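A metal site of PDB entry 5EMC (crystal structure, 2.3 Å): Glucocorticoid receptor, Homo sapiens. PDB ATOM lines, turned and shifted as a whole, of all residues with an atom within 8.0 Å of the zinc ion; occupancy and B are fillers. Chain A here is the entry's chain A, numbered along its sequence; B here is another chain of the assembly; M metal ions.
The zinc ion is bound by SG of Cys 67 (2.3 Å), SG of Cys 57 of chain A (2.3 Å), SG of Cys 51 (2.4 Å) and SG of Cys 70 (2.4 Å). The zinc ion has four donor atoms within binding distance.
Of the 22 residues printed, 4 come within 4 Å of the zinc ion. Along chain A the residues within 4 Å of the zinc ion span positions 51 to 70.
N of Asn 55 lies close to SG of Cys 51, at 3.2 Å. The side-chain sulfur of Cys 51 lies close to the backbone NH of Gly 53 of chain A (3.1 Å). The side-chain sulfur (SG) of Cys 51 lies close to the backbone NH (N) of Arg 54 (3.6 Å). The side-chain sulfur (SG) of Cys 70 sits close to the backbone NH (N) of Asp 56 (3.6 Å). The guanidinium group (NH1) of Arg 73 lies close to the side-chain sulfur (SG) of Cys 70, at 3.3 Å.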
ATOM      1  N   LEU A  50      14.979 -11.994 -19.803  1.00  0.00           N
ATOM      2  CA  LEU A  50      14.099 -12.753 -18.931  1.00  0.00           C
ATOM      3  C   LEU A  50      14.180 -12.274 -17.489  1.00  0.00           C
ATOM      4  O   LEU A  50      15.246 -12.281 -16.875  1.00  0.00           O
ATOM      5  CB  LEU A  50      14.429 -14.247 -18.981  1.00  0.00           C
ATOM      6  CG  LEU A  50      13.651 -15.123 -17.993  1.00  0.00           C
ATOM      7  CD1 LEU A  50      12.147 -14.924 -18.169  1.00  0.00           C
ATOM      8  CD2 LEU A  50      14.033 -16.604 -18.131  1.00  0.00           C
ATOM      9  N   CYS A  51      13.030 -11.861 -16.960  1.00  0.00           N
ATOM     10  CA  CYS A  51      12.932 -11.456 -15.560  1.00  0.00           C
ATOM     11  C   CYS A  51      13.122 -12.669 -14.642  1.00  0.00           C
ATOM     12  O   CYS A  51      12.642 -13.751 -14.936  1.00  0.00           O
ATOM     13  CB  CYS A  51      11.576 -10.817 -15.306  1.00  0.00           C
ATOM     14  SG  CYS A  51      11.326 -10.308 -13.610  1.00  0.00           S
ATOM     15  N   ALA A  52      13.852 -12.490 -13.535  1.00  0.00           N
ATOM     16  CA  ALA A  52      14.008 -13.557 -12.551  1.00  0.00           C
ATOM     17  C   ALA A  52      12.886 -13.502 -11.515  1.00  0.00           C
ATOM     18  O   ALA A  52      12.787 -14.397 -10.682  1.00  0.00           O
ATOM     19  CB  ALA A  52      15.366 -13.477 -11.858  1.00  0.00           C
ATOM     20  N   GLY A  53      12.058 -12.468 -11.583  1.00  0.00           N
ATOM     21  CA  GLY A  53      11.005 -12.263 -10.603  1.00  0.00           C
ATOM     22  C   GLY A  53       9.590 -12.441 -11.111  1.00  0.00           C
ATOM     23  O   GLY A  53       9.168 -13.557 -11.451  1.00  0.00           O
ATOM     24  N   ARG A  54       8.846 -11.348 -11.144  1.00  0.00           N
ATOM     25  CA  ARG A  54       7.433 -11.384 -11.525  1.00  0.00           C
ATOM     26  C   ARG A  54       7.125 -10.289 -12.526  1.00  0.00           C
ATOM     27  O   ARG A  54       5.983  -9.824 -12.594  1.00  0.00           O
ATOM     28  CB  ARG A  54       6.531 -11.240 -10.295  1.00  0.00           C
ATOM     29  CG  ARG A  54       6.713 -12.317  -9.228  1.00  0.00           C
ATOM     30  CD  ARG A  54       6.136 -11.858  -7.904  1.00  0.00           C
ATOM     31  NE  ARG A  54       6.114 -12.926  -6.907  1.00  0.00           N
ATOM     32  CZ  ARG A  54       7.137 -13.241  -6.121  1.00  0.00           C
ATOM     33  NH1 ARG A  54       8.281 -12.570  -6.213  1.00  0.00           N
ATOM     34  NH2 ARG A  54       7.023 -14.227  -5.248  1.00  0.00           N
ATOM     35  N   ASN A  55       8.139  -9.884 -13.288  1.00  0.00           N
ATOM     36  CA  ASN A  55       8.017  -8.804 -14.271  1.00  0.00           C
ATOM     37  C   ASN A  55       7.612  -7.471 -13.659  1.00  0.00           C
ATOM     38  O   ASN A  55       6.958  -6.665 -14.306  1.00  0.00           O
ATOM     39  CB  ASN A  55       7.033  -9.191 -15.372  1.00  0.00           C
ATOM     40  CG  ASN A  55       7.701  -9.881 -16.540  1.00  0.00           C
ATOM     41  OD1 ASN A  55       8.911  -9.770 -16.715  1.00  0.00           O
ATOM     42  ND2 ASN A  55       6.916 -10.584 -17.354  1.00  0.00           N
ATOM     43  N   ASP A  56       7.992  -7.224 -12.403  1.00  0.00           N
ATOM     44  CA  ASP A  56       7.689  -5.961 -11.747  1.00  0.00           C
ATOM     45  C   ASP A  56       8.831  -5.542 -10.827  1.00  0.00           C
ATOM     46  O   ASP A  56       8.607  -4.989  -9.758  1.00  0.00           O
ATOM     47  CB  ASP A  56       6.374  -6.039 -10.966  1.00  0.00           C
ATOM     48  CG  ASP A  56       6.420  -7.062  -9.825  1.00  0.00           C
ATOM     49  OD1 ASP A  56       7.400  -7.855  -9.733  1.00  0.00           O
ATOM     50  OD2 ASP A  56       5.465  -7.073  -9.013  1.00  0.00           O
ATOM     51  N   CYS A  57      10.059  -5.811 -11.257  1.00  0.00           N
ATOM     52  CA  CYS A  57      11.253  -5.460 -10.501  1.00  0.00           C
ATOM     53  C   CYS A  57      11.389  -3.974 -10.190  1.00  0.00           C
ATOM     54  O   CYS A  57      10.926  -3.130 -10.960  1.00  0.00           O
ATOM     55  CB  CYS A  57      12.497  -5.920 -11.256  1.00  0.00           C
ATOM     56  SG  CYS A  57      12.620  -7.693 -11.291  1.00  0.00           S
ATOM     57  N   ILE A  58      12.033  -3.669  -9.068  1.00  0.00           N
ATOM     58  CA  ILE A  58      12.358  -2.288  -8.709  1.00  0.00           C
ATOM     59  C   ILE A  58      13.518  -1.841  -9.573  1.00  0.00           C
ATOM     60  O   ILE A  58      14.518  -2.539  -9.670  1.00  0.00           O
ATOM     61  CB  ILE A  58      12.751  -2.144  -7.209  1.00  0.00           C
ATOM     62  CG1 ILE A  58      11.640  -2.652  -6.291  1.00  0.00           C
ATOM     63  CG2 ILE A  58      13.109  -0.683  -6.879  1.00  0.00           C
ATOM     64  CD1 ILE A  58      10.355  -1.884  -6.393  1.00  0.00           C
ATOM     65  N   ILE A  59      13.394  -0.680 -10.205  1.00  0.00           N
ATOM     66  CA  ILE A  59      14.474  -0.179 -11.037  1.00  0.00           C
ATOM     67  C   ILE A  59      14.969   1.165 -10.493  1.00  0.00           C
ATOM     68  O   ILE A  59      14.357   2.202 -10.727  1.00  0.00           O
ATOM     69  CB  ILE A  59      14.036  -0.021 -12.503  1.00  0.00           C
ATOM     70  CG1 ILE A  59      13.407  -1.315 -13.010  1.00  0.00           C
ATOM     71  CG2 ILE A  59      15.220   0.347 -13.380  1.00  0.00           C
ATOM     72  CD1 ILE A  59      14.384  -2.471 -13.147  1.00  0.00           C
ATOM     73  N   ARG A  63      19.555  -1.299  -8.859  1.00  0.00           N
ATOM     74  CA  ARG A  63      18.764  -2.448  -9.300  1.00  0.00           C
ATOM     75  C   ARG A  63      18.471  -2.478 -10.808  1.00  0.00           C
ATOM     76  O   ARG A  63      18.032  -3.505 -11.342  1.00  0.00           O
ATOM     77  CB  ARG A  63      17.441  -2.473  -8.524  1.00  0.00           C
ATOM     78  CG  ARG A  63      17.632  -2.584  -7.014  1.00  0.00           C
ATOM     79  CD  ARG A  63      16.336  -2.323  -6.244  1.00  0.00           C
ATOM     80  NE  ARG A  63      16.399  -2.869  -4.890  1.00  0.00           N
ATOM     81  CZ  ARG A  63      16.672  -2.167  -3.798  1.00  0.00           C
ATOM     82  NH1 ARG A  63      16.879  -0.859  -3.876  1.00  0.00           N
ATOM     83  NH2 ARG A  63      16.706  -2.773  -2.625  1.00  0.00           N
ATOM     84  N   ASN A  66      20.006  -5.323 -12.573  1.00  0.00           N
ATOM     85  CA  ASN A  66      19.531  -6.665 -12.205  1.00  0.00           C
ATOM     86  C   ASN A  66      18.640  -7.262 -13.281  1.00  0.00           C
ATOM     87  O   ASN A  66      18.788  -8.435 -13.670  1.00  0.00           O
ATOM     88  CB  ASN A  66      18.762  -6.627 -10.883  1.00  0.00           C
ATOM     89  CG  ASN A  66      19.675  -6.426  -9.676  1.00  0.00           C
ATOM     90  OD1 ASN A  66      20.830  -6.019  -9.796  1.00  0.00           O
ATOM     91  ND2 ASN A  66      19.152  -6.745  -8.494  1.00  0.00           N
ATOM     92  N   CYS A  67      17.719  -6.442 -13.787  1.00  0.00           N
ATOM     93  CA  CYS A  67      16.680  -6.917 -14.658  1.00  0.00           C
ATOM     94  C   CYS A  67      16.491  -6.046 -15.912  1.00  0.00           C
ATOM     95  O   CYS A  67      15.690  -5.111 -15.891  1.00  0.00           O
ATOM     96  CB  CYS A  67      15.374  -6.994 -13.883  1.00  0.00           C
ATOM     97  SG  CYS A  67      14.150  -7.966 -14.699  1.00  0.00           S
ATOM     98  N   PRO A  68      17.216  -6.338 -16.993  1.00  0.00           N
ATOM     99  CA  PRO A  68      17.055  -5.581 -18.239  1.00  0.00           C
ATOM    100  C   PRO A  68      15.657  -5.745 -18.856  1.00  0.00           C
ATOM    101  O   PRO A  68      15.184  -4.838 -19.532  1.00  0.00           O
ATOM    102  CB  PRO A  68      18.133  -6.156 -19.160  1.00  0.00           C
ATOM    103  CG  PRO A  68      18.626  -7.434 -18.472  1.00  0.00           C
ATOM    104  CD  PRO A  68      18.408  -7.217 -17.031  1.00  0.00           C
ATOM    105  N   ALA A  69      14.996  -6.875 -18.609  1.00  0.00           N
ATOM    106  CA  ALA A  69      13.618  -7.057 -19.055  1.00  0.00           C
ATOM    107  C   ALA A  69      12.678  -6.021 -18.456  1.00  0.00           C
ATOM    108  O   ALA A  69      11.906  -5.372 -19.173  1.00  0.00           O
ATOM    109  CB  ALA A  69      13.123  -8.464 -18.711  1.00  0.00           C
ATOM    110  N   CYS A  70      12.723  -5.868 -17.134  1.00  0.00           N
ATOM    111  CA  CYS A  70      11.919  -4.857 -16.445  1.00  0.00           C
ATOM    112  C   CYS A  70      12.394  -3.446 -16.742  1.00  0.00           C
ATOM    113  O   CYS A  70      11.607  -2.507 -16.796  1.00  0.00           O
ATOM    114  CB  CYS A  70      11.924  -5.097 -14.937  1.00  0.00           C
ATOM    115  SG  CYS A  70      10.808  -6.416 -14.409  1.00  0.00           S
ATOM    116  N   ARG A  71      13.696  -3.295 -16.952  1.00  0.00           N
ATOM    117  CA  ARG A  71      14.254  -1.992 -17.246  1.00  0.00           C
ATOM    118  C   ARG A  71      13.784  -1.509 -18.610  1.00  0.00           C
ATOM    119  O   ARG A  71      13.394  -0.352 -18.763  1.00  0.00           O
ATOM    120  CB  ARG A  71      15.777  -2.043 -17.191  1.00  0.00           C
ATOM    121  CG  ARG A  71      16.448  -0.699 -17.362  1.00  0.00           C
ATOM    122  CD  ARG A  71      17.959  -0.896 -17.412  1.00  0.00           C
ATOM    123  NE  ARG A  71      18.687   0.370 -17.419  1.00  0.00           N
ATOM    124  CZ  ARG A  71      20.004   0.450 -17.395  1.00  0.00           C
ATOM    125  NH1 ARG A  71      20.727  -0.663 -17.363  1.00  0.00           N
ATOM    126  NH2 ARG A  71      20.606   1.626 -17.395  1.00  0.00           N
ATOM    127  N   ARG A  73      11.196  -2.566 -20.151  1.00  0.00           N
ATOM    128  CA  ARG A  73       9.747  -2.416 -20.102  1.00  0.00           C
ATOM    129  C   ARG A  73       9.364  -1.046 -19.526  1.00  0.00           C
ATOM    130  O   ARG A  73       8.499  -0.368 -20.058  1.00  0.00           O
ATOM    131  CB  ARG A  73       9.121  -3.557 -19.279  1.00  0.00           C
ATOM    132  CG  ARG A  73       7.772  -3.257 -18.611  1.00  0.00           C
ATOM    133  CD  ARG A  73       7.230  -4.442 -17.751  1.00  0.00           C
ATOM    134  NE  ARG A  73       8.292  -5.328 -17.275  1.00  0.00           N
ATOM    135  CZ  ARG A  73       8.596  -6.513 -17.814  1.00  0.00           C
ATOM    136  NH1 ARG A  73       9.577  -7.255 -17.313  1.00  0.00           N
ATOM    137  NH2 ARG A  73       7.930  -6.950 -18.877  1.00  0.00           N
ATOM    138  N   ALA B  52      15.930  -6.836  -6.723  1.00  0.00           N
ATOM    139  CA  ALA B  52      14.935  -5.922  -7.318  1.00  0.00           C
ATOM    140  C   ALA B  52      13.534  -6.500  -7.271  1.00  0.00           C
ATOM    141  O   ALA B  52      12.589  -5.825  -7.643  1.00  0.00           O
ATOM    142  CB  ALA B  52      15.292  -5.592  -8.745  1.00  0.00           C
ATOM    143  N   GLY B  53      13.413  -7.753  -6.818  1.00  0.00           N
ATOM    144  CA  GLY B  53      12.122  -8.399  -6.654  1.00  0.00           C
ATOM    145  C   GLY B  53      11.723  -8.553  -5.189  1.00  0.00           C
ATOM    146  O   GLY B  53      11.669  -7.568  -4.453  1.00  0.00           O
ATOM    147  N   CYS B  57      14.106 -14.540  -5.957  1.00  0.00           N
ATOM    148  CA  CYS B  57      14.298 -14.616  -7.399  1.00  0.00           C
ATOM    149  C   CYS B  57      14.647 -16.041  -7.843  1.00  0.00           C
ATOM    150  O   CYS B  57      15.262 -16.792  -7.095  1.00  0.00           O
ATOM    151  CB  CYS B  57      15.381 -13.631  -7.821  1.00  0.00           C
ATOM    152  SG  CYS B  57      14.935 -11.878  -7.647  1.00  0.00           S
ATOM    153  N   ASN B  66      20.979 -12.412 -12.961  1.00  0.00           N
ATOM    154  CA  ASN B  66      20.033 -11.318 -12.683  1.00  0.00           C
ATOM    155  C   ASN B  66      20.136 -10.833 -11.244  1.00  0.00           C
ATOM    156  O   ASN B  66      20.125  -9.643 -10.976  1.00  0.00           O
ATOM    157  CB  ASN B  66      18.570 -11.746 -12.938  1.00  0.00           C
ATOM    158  CG  ASN B  66      18.261 -11.948 -14.404  1.00  0.00           C
ATOM    159  OD1 ASN B  66      19.132 -12.274 -15.198  1.00  0.00           O
ATOM    160  ND2 ASN B  66      16.996 -11.761 -14.772  1.00  0.00           N
HETATM  161 ZN    ZN M   1      12.223  -8.113 -13.506  1.00  0.00          ZN
